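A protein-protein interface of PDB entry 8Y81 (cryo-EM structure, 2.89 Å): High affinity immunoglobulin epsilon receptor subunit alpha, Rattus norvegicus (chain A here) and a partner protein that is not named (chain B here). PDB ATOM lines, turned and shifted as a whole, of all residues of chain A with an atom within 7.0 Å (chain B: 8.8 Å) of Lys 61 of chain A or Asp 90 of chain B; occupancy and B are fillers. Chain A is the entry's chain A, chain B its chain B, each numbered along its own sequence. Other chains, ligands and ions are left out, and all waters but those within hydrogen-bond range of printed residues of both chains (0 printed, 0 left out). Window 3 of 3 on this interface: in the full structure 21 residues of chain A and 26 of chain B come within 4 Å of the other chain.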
ATOM      1  N   CYS A  49       7.041  10.411  19.459  1.00  0.00           N
ATOM      2  CA  CYS A  49       7.326  11.679  18.801  1.00  0.00           C
ATOM      3  C   CYS A  49       5.977  12.262  18.351  1.00  0.00           C
ATOM      4  O   CYS A  49       4.993  12.100  19.079  1.00  0.00           O
ATOM      5  CB  CYS A  49       8.331  11.487  17.667  1.00  0.00           C
ATOM      6  SG  CYS A  49       8.946  13.044  17.051  1.00  0.00           S
ATOM      7  N   ASN A  58      13.394   3.725  11.903  1.00  0.00           N
ATOM      8  CA  ASN A  58      14.381   4.469  11.109  1.00  0.00           C
ATOM      9  C   ASN A  58      13.817   5.779  10.561  1.00  0.00           C
ATOM     10  O   ASN A  58      14.126   6.188   9.441  1.00  0.00           O
ATOM     11  CB  ASN A  58      14.951   3.607   9.978  1.00  0.00           C
ATOM     12  CG  ASN A  58      16.146   2.782  10.418  1.00  0.00           C
ATOM     13  OD1 ASN A  58      16.992   3.249  11.180  1.00  0.00           O
ATOM     14  ND2 ASN A  58      16.220   1.546   9.936  1.00  0.00           N
ATOM     15  N   SER A  59      12.980   6.448  11.359  1.00  0.00           N
ATOM     16  CA  SER A  59      12.355   7.687  10.914  1.00  0.00           C
ATOM     17  C   SER A  59      12.314   8.760  11.995  1.00  0.00           C
ATOM     18  O   SER A  59      11.625   9.770  11.812  1.00  0.00           O
ATOM     19  CB  SER A  59      10.933   7.418  10.410  1.00  0.00           C
ATOM     20  OG  SER A  59      10.920   6.403   9.423  1.00  0.00           O
ATOM     21  N   THR A  60      13.015   8.578  13.112  1.00  0.00           N
ATOM     22  CA  THR A  60      13.004   9.541  14.204  1.00  0.00           C
ATOM     23  C   THR A  60      14.389   9.599  14.824  1.00  0.00           C
ATOM     24  O   THR A  60      14.946   8.564  15.192  1.00  0.00           O
ATOM     25  CB  THR A  60      11.966   9.159  15.267  1.00  0.00           C
ATOM     26  OG1 THR A  60      10.667   9.096  14.668  1.00  0.00           O
ATOM     27  CG2 THR A  60      11.938  10.175  16.384  1.00  0.00           C
ATOM     28  N   LYS A  61      14.944  10.797  14.938  1.00  0.00           N
ATOM     29  CA  LYS A  61      16.214  11.015  15.611  1.00  0.00           C
ATOM     30  C   LYS A  61      15.927  11.308  17.076  1.00  0.00           C
ATOM     31  O   LYS A  61      15.194  12.249  17.391  1.00  0.00           O
ATOM     32  CB  LYS A  61      16.975  12.167  14.959  1.00  0.00           C
ATOM     33  CG  LYS A  61      18.301  12.496  15.605  1.00  0.00           C
ATOM     34  CD  LYS A  61      18.977  13.637  14.872  1.00  0.00           C
ATOM     35  CE  LYS A  61      20.329  13.955  15.473  1.00  0.00           C
ATOM     36  NZ  LYS A  61      21.043  15.014  14.713  1.00  0.00           N
ATOM     37  N   TRP A  62      16.486  10.494  17.964  1.00  0.00           N
ATOM     38  CA  TRP A  62      16.225  10.587  19.392  1.00  0.00           C
ATOM     39  C   TRP A  62      17.467  11.108  20.095  1.00  0.00           C
ATOM     40  O   TRP A  62      18.563  10.574  19.902  1.00  0.00           O
ATOM     41  CB  TRP A  62      15.827   9.225  19.959  1.00  0.00           C
ATOM     42  CG  TRP A  62      14.388   8.895  19.758  1.00  0.00           C
ATOM     43  CD1 TRP A  62      13.864   8.041  18.838  1.00  0.00           C
ATOM     44  CD2 TRP A  62      13.283   9.415  20.494  1.00  0.00           C
ATOM     45  NE1 TRP A  62      12.502   7.996  18.952  1.00  0.00           N
ATOM     46  CE2 TRP A  62      12.119   8.834  19.965  1.00  0.00           C
ATOM     47  CE3 TRP A  62      13.164  10.319  21.551  1.00  0.00           C
ATOM     48  CZ2 TRP A  62      10.858   9.125  20.455  1.00  0.00           C
ATOM     49  CZ3 TRP A  62      11.916  10.601  22.035  1.00  0.00           C
ATOM     50  CH2 TRP A  62      10.778  10.012  21.487  1.00  0.00           C
ATOM     51  N   ILE A  63      17.298  12.148  20.903  1.00  0.00           N
ATOM     52  CA  ILE A  63      18.379  12.734  21.683  1.00  0.00           C
ATOM     53  C   ILE A  63      18.022  12.557  23.148  1.00  0.00           C
ATOM     54  O   ILE A  63      16.995  13.070  23.606  1.00  0.00           O
ATOM     55  CB  ILE A  63      18.602  14.219  21.350  1.00  0.00           C
ATOM     56  CG1 ILE A  63      19.065  14.405  19.905  1.00  0.00           C
ATOM     57  CG2 ILE A  63      19.611  14.832  22.292  1.00  0.00           C
ATOM     58  CD1 ILE A  63      17.967  14.815  18.948  1.00  0.00           C
ATOM     59  N   ILE A  68      22.937  11.703  21.088  1.00  0.00           N
ATOM     60  CA  ILE A  68      22.039  11.090  20.113  1.00  0.00           C
ATOM     61  C   ILE A  68      22.021   9.584  20.334  1.00  0.00           C
ATOM     62  O   ILE A  68      23.049   8.910  20.206  1.00  0.00           O
ATOM     63  CB  ILE A  68      22.449  11.430  18.671  1.00  0.00           C
ATOM     64  CG1 ILE A  68      22.369  12.938  18.369  1.00  0.00           C
ATOM     65  CG2 ILE A  68      21.589  10.663  17.684  1.00  0.00           C
ATOM     66  CD1 ILE A  68      23.628  13.771  18.653  1.00  0.00           C
ATOM     67  N   SER A  69      20.851   9.051  20.659  1.00  0.00           N
ATOM     68  CA  SER A  69      20.700   7.629  20.918  1.00  0.00           C
ATOM     69  C   SER A  69      20.491   6.862  19.616  1.00  0.00           C
ATOM     70  O   SER A  69      20.051   7.409  18.604  1.00  0.00           O
ATOM     71  CB  SER A  69      19.531   7.374  21.864  1.00  0.00           C
ATOM     72  OG  SER A  69      18.321   7.233  21.144  1.00  0.00           O
ATOM     73  N   VAL A  71      18.316   4.539  19.165  1.00  0.00           N
ATOM     74  CA  VAL A  71      16.909   4.224  18.942  1.00  0.00           C
ATOM     75  C   VAL A  71      16.370   5.157  17.869  1.00  0.00           C
ATOM     76  O   VAL A  71      16.362   6.381  18.036  1.00  0.00           O
ATOM     77  CB  VAL A  71      16.103   4.350  20.240  1.00  0.00           C
ATOM     78  CG1 VAL A  71      14.638   4.074  19.972  1.00  0.00           C
ATOM     79  CG2 VAL A  71      16.644   3.400  21.289  1.00  0.00           C
ATOM     80  N   LYS A  72      15.930   4.584  16.751  1.00  0.00           N
ATOM     81  CA  LYS A  72      15.488   5.378  15.614  1.00  0.00           C
ATOM     82  C   LYS A  72      14.026   5.146  15.263  1.00  0.00           C
ATOM     83  O   LYS A  72      13.561   5.648  14.234  1.00  0.00           O
ATOM     84  CB  LYS A  72      16.381   5.106  14.403  1.00  0.00           C
ATOM     85  CG  LYS A  72      17.801   5.601  14.599  1.00  0.00           C
ATOM     86  CD  LYS A  72      18.660   5.376  13.377  1.00  0.00           C
ATOM     87  CE  LYS A  72      20.088   5.810  13.647  1.00  0.00           C
ATOM     88  NZ  LYS A  72      20.188   7.283  13.828  1.00  0.00           N
ATOM     89  N   SER A  73      13.292   4.410  16.085  1.00  0.00           N
ATOM     90  CA  SER A  73      11.871   4.229  15.851  1.00  0.00           C
ATOM     91  C   SER A  73      11.097   5.453  16.322  1.00  0.00           C
ATOM     92  O   SER A  73      11.587   6.265  17.109  1.00  0.00           O
ATOM     93  CB  SER A  73      11.365   2.981  16.569  1.00  0.00           C
ATOM     94  OG  SER A  73      11.449   3.137  17.973  1.00  0.00           O
ATOM     95  N   ILE A  90      14.459  14.467  23.456  1.00  0.00           N
ATOM     96  CA  ILE A  90      14.063  15.235  22.279  1.00  0.00           C
ATOM     97  C   ILE A  90      13.860  14.252  21.132  1.00  0.00           C
ATOM     98  O   ILE A  90      14.687  13.361  20.929  1.00  0.00           O
ATOM     99  CB  ILE A  90      15.125  16.288  21.890  1.00  0.00           C
ATOM    100  CG1 ILE A  90      15.622  17.070  23.103  1.00  0.00           C
ATOM    101  CG2 ILE A  90      14.591  17.242  20.853  1.00  0.00           C
ATOM    102  CD1 ILE A  90      16.860  17.838  22.849  1.00  0.00           C
ATOM    103  N   CYS A  91      12.763  14.397  20.395  1.00  0.00           N
ATOM    104  CA  CYS A  91      12.581  13.645  19.162  1.00  0.00           C
ATOM    105  C   CYS A  91      12.668  14.598  17.981  1.00  0.00           C
ATOM    106  O   CYS A  91      12.471  15.806  18.122  1.00  0.00           O
ATOM    107  CB  CYS A  91      11.243  12.890  19.115  1.00  0.00           C
ATOM    108  SG  CYS A  91       9.768  13.865  18.735  1.00  0.00           S
ATOM    109  N   GLN A  92      12.991  14.045  16.818  1.00  0.00           N
ATOM    110  CA  GLN A  92      13.014  14.828  15.586  1.00  0.00           C
ATOM    111  C   GLN A  92      12.653  13.881  14.448  1.00  0.00           C
ATOM    112  O   GLN A  92      13.486  13.082  14.022  1.00  0.00           O
ATOM    113  CB  GLN A  92      14.376  15.471  15.367  1.00  0.00           C
ATOM    114  CG  GLN A  92      14.473  16.283  14.097  1.00  0.00           C
ATOM    115  CD  GLN A  92      15.860  16.819  13.865  1.00  0.00           C
ATOM    116  OE1 GLN A  92      16.781  16.529  14.625  1.00  0.00           O
ATOM    117  NE2 GLN A  92      16.024  17.605  12.812  1.00  0.00           N
ATOM    118  N   LYS A  93      11.414  13.959  13.983  1.00  0.00           N
ATOM    119  CA  LYS A  93      10.993  13.084  12.904  1.00  0.00           C
ATOM    120  C   LYS A  93      11.587  13.562  11.583  1.00  0.00           C
ATOM    121  O   LYS A  93      12.067  14.691  11.463  1.00  0.00           O
ATOM    122  CB  LYS A  93       9.470  13.032  12.831  1.00  0.00           C
ATOM    123  CG  LYS A  93       8.910  11.687  12.422  1.00  0.00           C
ATOM    124  CD  LYS A  93       7.473  11.529  12.875  1.00  0.00           C
ATOM    125  CE  LYS A  93       6.825  10.332  12.206  1.00  0.00           C
ATOM    126  NZ  LYS A  93       7.598   9.082  12.442  1.00  0.00           N
ATOM    127  N   GLN A  94      11.571  12.676  10.589  1.00  0.00           N
ATOM    128  CA  GLN A  94      12.138  12.996   9.284  1.00  0.00           C
ATOM    129  C   GLN A  94      11.275  14.038   8.586  1.00  0.00           C
ATOM    130  O   GLN A  94      10.091  13.802   8.324  1.00  0.00           O
ATOM    131  CB  GLN A  94      12.255  11.735   8.431  1.00  0.00           C
ATOM    132  CG  GLN A  94      13.610  11.049   8.523  1.00  0.00           C
ATOM    133  CD  GLN A  94      14.664  11.710   7.653  1.00  0.00           C
ATOM    134  OE1 GLN A  94      14.353  12.539   6.799  1.00  0.00           O
ATOM    135  NE2 GLN A  94      15.922  11.344   7.869  1.00  0.00           N
ATOM    136  N   LYS A  98      13.353  19.858  15.630  1.00  0.00           N
ATOM    137  CA  LYS A  98      13.605  19.264  16.934  1.00  0.00           C
ATOM    138  C   LYS A  98      12.495  19.636  17.905  1.00  0.00           C
ATOM    139  O   LYS A  98      11.873  20.695  17.798  1.00  0.00           O
ATOM    140  CB  LYS A  98      14.957  19.705  17.489  1.00  0.00           C
ATOM    141  CG  LYS A  98      16.124  18.929  16.922  1.00  0.00           C
ATOM    142  CD  LYS A  98      17.340  19.020  17.814  1.00  0.00           C
ATOM    143  CE  LYS A  98      18.545  18.402  17.142  1.00  0.00           C
ATOM    144  NZ  LYS A  98      19.746  18.470  18.005  1.00  0.00           N
ATOM    145  N   THR B  85      23.622  23.075  22.326  1.00  0.00           N
ATOM    146  CA  THR B  85      23.291  23.048  20.907  1.00  0.00           C
ATOM    147  C   THR B  85      22.601  21.766  20.462  1.00  0.00           C
ATOM    148  O   THR B  85      22.134  21.704  19.321  1.00  0.00           O
ATOM    149  CB  THR B  85      24.553  23.265  20.072  1.00  0.00           C
ATOM    150  OG1 THR B  85      25.551  22.312  20.456  1.00  0.00           O
ATOM    151  CG2 THR B  85      25.090  24.666  20.294  1.00  0.00           C
ATOM    152  N   SER B  86      22.533  20.743  21.312  1.00  0.00           N
ATOM    153  CA  SER B  86      21.756  19.558  20.978  1.00  0.00           C
ATOM    154  C   SER B  86      20.259  19.797  21.090  1.00  0.00           C
ATOM    155  O   SER B  86      19.478  19.051  20.492  1.00  0.00           O
ATOM    156  CB  SER B  86      22.143  18.395  21.885  1.00  0.00           C
ATOM    157  OG  SER B  86      21.372  18.432  23.069  1.00  0.00           O
ATOM    158  N   ASP B  87      19.844  20.818  21.842  1.00  0.00           N
ATOM    159  CA  ASP B  87      18.432  21.119  22.018  1.00  0.00           C
ATOM    160  C   ASP B  87      17.812  21.750  20.785  1.00  0.00           C
ATOM    161  O   ASP B  87      16.585  21.757  20.655  1.00  0.00           O
ATOM    162  CB  ASP B  87      18.241  22.073  23.196  1.00  0.00           C
ATOM    163  CG  ASP B  87      18.556  21.434  24.521  1.00  0.00           C
ATOM    164  OD1 ASP B  87      18.388  20.209  24.639  1.00  0.00           O
ATOM    165  OD2 ASP B  87      18.962  22.160  25.450  1.00  0.00           O
ATOM    166  N   PHE B  88      18.633  22.279  19.884  1.00  0.00           N
ATOM    167  CA  PHE B  88      18.181  23.099  18.777  1.00  0.00           C
ATOM    168  C   PHE B  88      18.660  22.503  17.464  1.00  0.00           C
ATOM    169  O   PHE B  88      19.565  21.667  17.429  1.00  0.00           O
ATOM    170  CB  PHE B  88      18.680  24.533  18.943  1.00  0.00           C
ATOM    171  CG  PHE B  88      18.505  25.056  20.331  1.00  0.00           C
ATOM    172  CD1 PHE B  88      17.253  25.424  20.788  1.00  0.00           C
ATOM    173  CD2 PHE B  88      19.580  25.145  21.196  1.00  0.00           C
ATOM    174  CE1 PHE B  88      17.081  25.887  22.071  1.00  0.00           C
ATOM    175  CE2 PHE B  88      19.412  25.608  22.479  1.00  0.00           C
ATOM    176  CZ  PHE B  88      18.163  25.978  22.914  1.00  0.00           C
ATOM    177  N   ASP B  89      18.026  22.942  16.382  1.00  0.00           N
ATOM    178  CA  ASP B  89      18.235  22.328  15.082  1.00  0.00           C
ATOM    179  C   ASP B  89      19.592  22.697  14.500  1.00  0.00           C
ATOM    180  O   ASP B  89      20.172  23.737  14.821  1.00  0.00           O
ATOM    181  CB  ASP B  89      17.128  22.750  14.129  1.00  0.00           C
ATOM    182  CG  ASP B  89      15.815  22.105  14.465  1.00  0.00           C
ATOM    183  OD1 ASP B  89      15.535  21.014  13.929  1.00  0.00           O
ATOM    184  OD2 ASP B  89      15.068  22.680  15.280  1.00  0.00           O
ATOM    185  N   ASP B  90      20.097  21.827  13.630  1.00  0.00           N
ATOM    186  CA  ASP B  90      21.380  22.060  12.987  1.00  0.00           C
ATOM    187  C   ASP B  90      21.275  22.975  11.778  1.00  0.00           C
ATOM    188  O   ASP B  90      22.306  23.315  11.188  1.00  0.00           O
ATOM    189  CB  ASP B  90      22.005  20.727  12.579  1.00  0.00           C
ATOM    190  CG  ASP B  90      21.968  19.706  13.694  1.00  0.00           C
ATOM    191  OD1 ASP B  90      22.491  20.006  14.787  1.00  0.00           O
ATOM    192  OD2 ASP B  90      21.413  18.606  13.483  1.00  0.00           O
ATOM    193  N   GLU B  91      20.065  23.362  11.384  1.00  0.00           N
ATOM    194  CA  GLU B  91      19.873  24.392  10.375  1.00  0.00           C
ATOM    195  C   GLU B  91      19.511  25.743  10.967  1.00  0.00           C
ATOM    196  O   GLU B  91      19.815  26.770  10.358  1.00  0.00           O
ATOM    197  CB  GLU B  91      18.810  23.956   9.357  1.00  0.00           C
ATOM    198  CG  GLU B  91      17.418  23.698   9.907  1.00  0.00           C
ATOM    199  CD  GLU B  91      17.225  22.254  10.348  1.00  0.00           C
ATOM    200  OE1 GLU B  91      18.230  21.533  10.513  1.00  0.00           O
ATOM    201  OE2 GLU B  91      16.067  21.828  10.516  1.00  0.00           O
ATOM    202  N   VAL B  92      18.881  25.766  12.140  1.00  0.00           N
ATOM    203  CA  VAL B  92      18.753  27.005  12.900  1.00  0.00           C
ATOM    204  C   VAL B  92      20.122  27.462  13.389  1.00  0.00           C
ATOM    205  O   VAL B  92      20.462  28.649  13.323  1.00  0.00           O
ATOM    206  CB  VAL B  92      17.756  26.798  14.054  1.00  0.00           C
ATOM    207  CG1 VAL B  92      17.912  27.848  15.137  1.00  0.00           C
ATOM    208  CG2 VAL B  92      16.352  26.809  13.517  1.00  0.00           C
ATOM    209  N   LEU B  93      20.947  26.519  13.842  1.00  0.00           N
ATOM    210  CA  LEU B  93      22.300  26.801  14.301  1.00  0.00           C
ATOM    211  C   LEU B  93      23.336  26.663  13.198  1.00  0.00           C
ATOM    212  O   LEU B  93      24.486  26.317  13.488  1.00  0.00           O
ATOM    213  CB  LEU B  93      22.656  25.886  15.471  1.00  0.00           C
ATOM    214  CG  LEU B  93      22.239  26.361  16.857  1.00  0.00           C
ATOM    215  CD1 LEU B  93      22.139  25.179  17.782  1.00  0.00           C
ATOM    216  CD2 LEU B  93      23.253  27.348  17.374  1.00  0.00           C
ATOM    217  N   LEU B  94      22.959  26.932  11.942  1.00  0.00           N
ATOM    218  CA  LEU B  94      23.886  26.813  10.816  1.00  0.00           C
ATOM    219  C   LEU B  94      25.027  27.821  10.917  1.00  0.00           C
ATOM    220  O   LEU B  94      26.108  27.594  10.363  1.00  0.00           O
ATOM    221  CB  LEU B  94      23.112  26.976   9.505  1.00  0.00           C
ATOM    222  CG  LEU B  94      23.799  27.197   8.156  1.00  0.00           C
ATOM    223  CD1 LEU B  94      24.649  25.998   7.802  1.00  0.00           C
ATOM    224  CD2 LEU B  94      22.778  27.465   7.079  1.00  0.00           C
ATOM    225  N   LEU B  95      24.805  28.926  11.632  1.00  0.00           N
ATOM    226  CA  LEU B  95      25.878  29.850  11.988  1.00  0.00           C
ATOM    227  C   LEU B  95      26.990  29.161  12.765  1.00  0.00           C
ATOM    228  O   LEU B  95      28.174  29.317  12.451  1.00  0.00           O
ATOM    229  CB  LEU B  95      25.297  30.987  12.819  1.00  0.00           C
ATOM    230  CG  LEU B  95      26.289  32.054  13.223  1.00  0.00           C
ATOM    231  CD1 LEU B  95      26.804  32.681  11.998  1.00  0.00           C
ATOM    232  CD2 LEU B  95      25.587  33.056  14.088  1.00  0.00           C
ATOM    233  N   TYR B  96      26.624  28.387  13.777  1.00  0.00           N
ATOM    234  CA  TYR B  96      27.603  27.779  14.663  1.00  0.00           C
ATOM    235  C   TYR B  96      28.038  26.404  14.177  1.00  0.00           C
ATOM    236  O   TYR B  96      29.192  26.018  14.391  1.00  0.00           O
ATOM    237  CB  TYR B  96      27.019  27.709  16.078  1.00  0.00           C
ATOM    238  CG  TYR B  96      27.818  26.917  17.084  1.00  0.00           C
ATOM    239  CD1 TYR B  96      28.937  27.466  17.696  1.00  0.00           C
ATOM    240  CD2 TYR B  96      27.435  25.632  17.448  1.00  0.00           C
ATOM    241  CE1 TYR B  96      29.665  26.751  18.626  1.00  0.00           C
ATOM    242  CE2 TYR B  96      28.159  24.907  18.374  1.00  0.00           C
ATOM    243  CZ  TYR B  96      29.269  25.472  18.961  1.00  0.00           C
ATOM    244  OH  TYR B  96      29.986  24.749  19.885  1.00  0.00           O
ATOM    245  N   ARG B  97      27.144  25.666  13.511  1.00  0.00           N
ATOM    246  CA  ARG B  97      27.498  24.344  13.005  1.00  0.00           C
ATOM    247  C   ARG B  97      28.450  24.432  11.822  1.00  0.00           C
ATOM    248  O   ARG B  97      29.292  23.547  11.643  1.00  0.00           O
ATOM    249  CB  ARG B  97      26.240  23.566  12.621  1.00  0.00           C
ATOM    250  CG  ARG B  97      25.367  23.190  13.806  1.00  0.00           C
ATOM    251  CD  ARG B  97      25.546  21.745  14.213  1.00  0.00           C
ATOM    252  NE  ARG B  97      26.749  21.562  15.020  1.00  0.00           N
ATOM    253  CZ  ARG B  97      26.794  21.709  16.340  1.00  0.00           C
ATOM    254  NH1 ARG B  97      25.702  22.046  17.010  1.00  0.00           N
ATOM    255  NH2 ARG B  97      27.936  21.524  16.989  1.00  0.00           N
ATOM    256  N   ALA B  98      28.342  25.483  11.009  1.00  0.00           N
ATOM    257  CA  ALA B  98      29.365  25.752  10.007  1.00  0.00           C
ATOM    258  C   ALA B  98      30.572  26.467  10.591  1.00  0.00           C
ATOM    259  O   ALA B  98      31.549  26.688   9.872  1.00  0.00           O
ATOM    260  CB  ALA B  98      28.799  26.579   8.853  1.00  0.00           C
ATOM    261  N   ASN B 151      21.044  31.161   6.890  1.00  0.00           N
ATOM    262  CA  ASN B 151      20.546  31.021   8.250  1.00  0.00           C
ATOM    263  C   ASN B 151      19.329  31.896   8.509  1.00  0.00           C
ATOM    264  O   ASN B 151      18.464  31.503   9.291  1.00  0.00           O
ATOM    265  CB  ASN B 151      21.640  31.322   9.265  1.00  0.00           C
ATOM    266  CG  ASN B 151      21.373  30.660  10.590  1.00  0.00           C
ATOM    267  OD1 ASN B 151      20.422  29.896  10.725  1.00  0.00           O
ATOM    268  ND2 ASN B 151      22.207  30.933  11.572  1.00  0.00           N
ATOM    269  N   ASN B 154      16.606  29.731   7.010  1.00  0.00           N
ATOM    270  CA  ASN B 154      16.266  28.635   7.914  1.00  0.00           C
ATOM    271  C   ASN B 154      15.538  29.138   9.152  1.00  0.00           C
ATOM    272  O   ASN B 154      14.638  28.465   9.665  1.00  0.00           O
ATOM    273  CB  ASN B 154      17.527  27.882   8.314  1.00  0.00           C
ATOM    274  CG  ASN B 154      18.188  27.194   7.145  1.00  0.00           C
ATOM    275  OD1 ASN B 154      17.587  27.034   6.085  1.00  0.00           O
ATOM    276  ND2 ASN B 154      19.432  26.780   7.331  1.00  0.00           N
ATOM    277  N   ASN B 155      15.901  30.325   9.637  1.00  0.00           N
ATOM    278  CA  ASN B 155      15.248  30.881  10.813  1.00  0.00           C
ATOM    279  C   ASN B 155      13.831  31.335  10.498  1.00  0.00           C
ATOM    280  O   ASN B 155      12.936  31.197  11.336  1.00  0.00           O
ATOM    281  CB  ASN B 155      16.081  32.034  11.363  1.00  0.00           C
ATOM    282  CG  ASN B 155      17.264  31.560  12.180  1.00  0.00           C
ATOM    283  OD1 ASN B 155      18.094  32.356  12.607  1.00  0.00           O
ATOM    284  ND2 ASN B 155      17.350  30.258  12.397  1.00  0.00           N
ATOM    285  N   TYR B 158      11.835  28.216  10.374  1.00  0.00           N
ATOM    286  CA  TYR B 158      11.509  27.780  11.727  1.00  0.00           C
ATOM    287  C   TYR B 158      10.393  28.626  12.328  1.00  0.00           C
ATOM    288  O   TYR B 158       9.440  28.092  12.903  1.00  0.00           O
ATOM    289  CB  TYR B 158      12.750  27.838  12.615  1.00  0.00           C
ATOM    290  CG  TYR B 158      12.613  27.069  13.913  1.00  0.00           C
ATOM    291  CD1 TYR B 158      12.955  25.731  13.980  1.00  0.00           C
ATOM    292  CD2 TYR B 158      12.143  27.682  15.068  1.00  0.00           C
ATOM    293  CE1 TYR B 158      12.840  25.025  15.149  1.00  0.00           C
ATOM    294  CE2 TYR B 158      12.022  26.982  16.244  1.00  0.00           C
ATOM    295  CZ  TYR B 158      12.372  25.654  16.276  1.00  0.00           C
ATOM    296  OH  TYR B 158      12.260  24.941  17.442  1.00  0.00           O
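The backbone carbonyl oxygen (O) of Gln 92 of chain A lies within hydrogen-bond range of the backbone NH (N) of Lys 61 of chain A, 2.9 Å away.
N of Ile 63 of chain A is in hydrogen-bond range of O of Ile 90 of chain A, 2.9 Å away.
The side-chain sulfur (SG) of Cys 91 of chain A is disulfide-bonded to the side-chain sulfur (SG) of Cys 49 of chain A (2.0 Å).
Of the printed residues of chain B, Lys 61 of chain A touches Asp 90.
Of the printed residues of chain B, Ile 90 of chain A touches Ser 86 and Asp 87.
Of the printed residues of chain B, Lys 98 of chain A touches Ser 86 (2.6 Å), Phe 88 (3.3 Å) and Asp 89 (3.0 Å).
Printed residues of chain A within 4 Å of Ser 86 of chain B: Ile 90 (3.7 Å) and Lys 98 (2.6 Å).
Of the printed residues of chain A, Asp 87 of chain B touches Ile 90 (3.3 Å).
Leu 93 of chain B touches none of the printed residues of chain A.
The nearest residue of chain B that does not touch Lys 61 of chain A is Ser 86 of chain B (7.2 Å).
The nearest residue of chain A that does not touch Asp 90 of chain B is Lys 98 of chain A (4.5 Å).
The nearest printed residue of chain B that does not touch Ile 90 of chain A is Phe 88 of chain B (5.6 Å).
The side-chain amino group (NZ) of Lys 61 of chain A lies within salt-bridge range of the side-chain carboxylate (OD2) of Asp 90 of chain B (3.8 Å).
The side-chain amino group of Lys 98 of chain A lies within hydrogen-bond range of the backbone carbonyl oxygen of Ser 86 of chain B.
The backbone carbonyl oxygen (O) of Phe 88 of chain B is in hydrogen-bond range of the side-chain amino group (NZ) of Lys 98 of chain A.
OD1 of Asp 89 of chain B lies within hydrogen-bond range of N of Lys 98 of chain A, at 3.0 Å.
Among the printed residues, merely in contact across the chains: Ile 90 of chain A with Ser 86 of chain B, Ile 90 of chain A with Asp 87 of chain B and Gln 92 of chain A with Asp 89 of chain B.
Of the 18 printed residues of chain A, 4 touch a printed residue of chain B.
Printed residues of chain A that touch a printed residue of chain B: Lys 61, Ile 90, Gln 92 and Lys 98.
Among the printed residues, 7 pairs touch across the chains.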
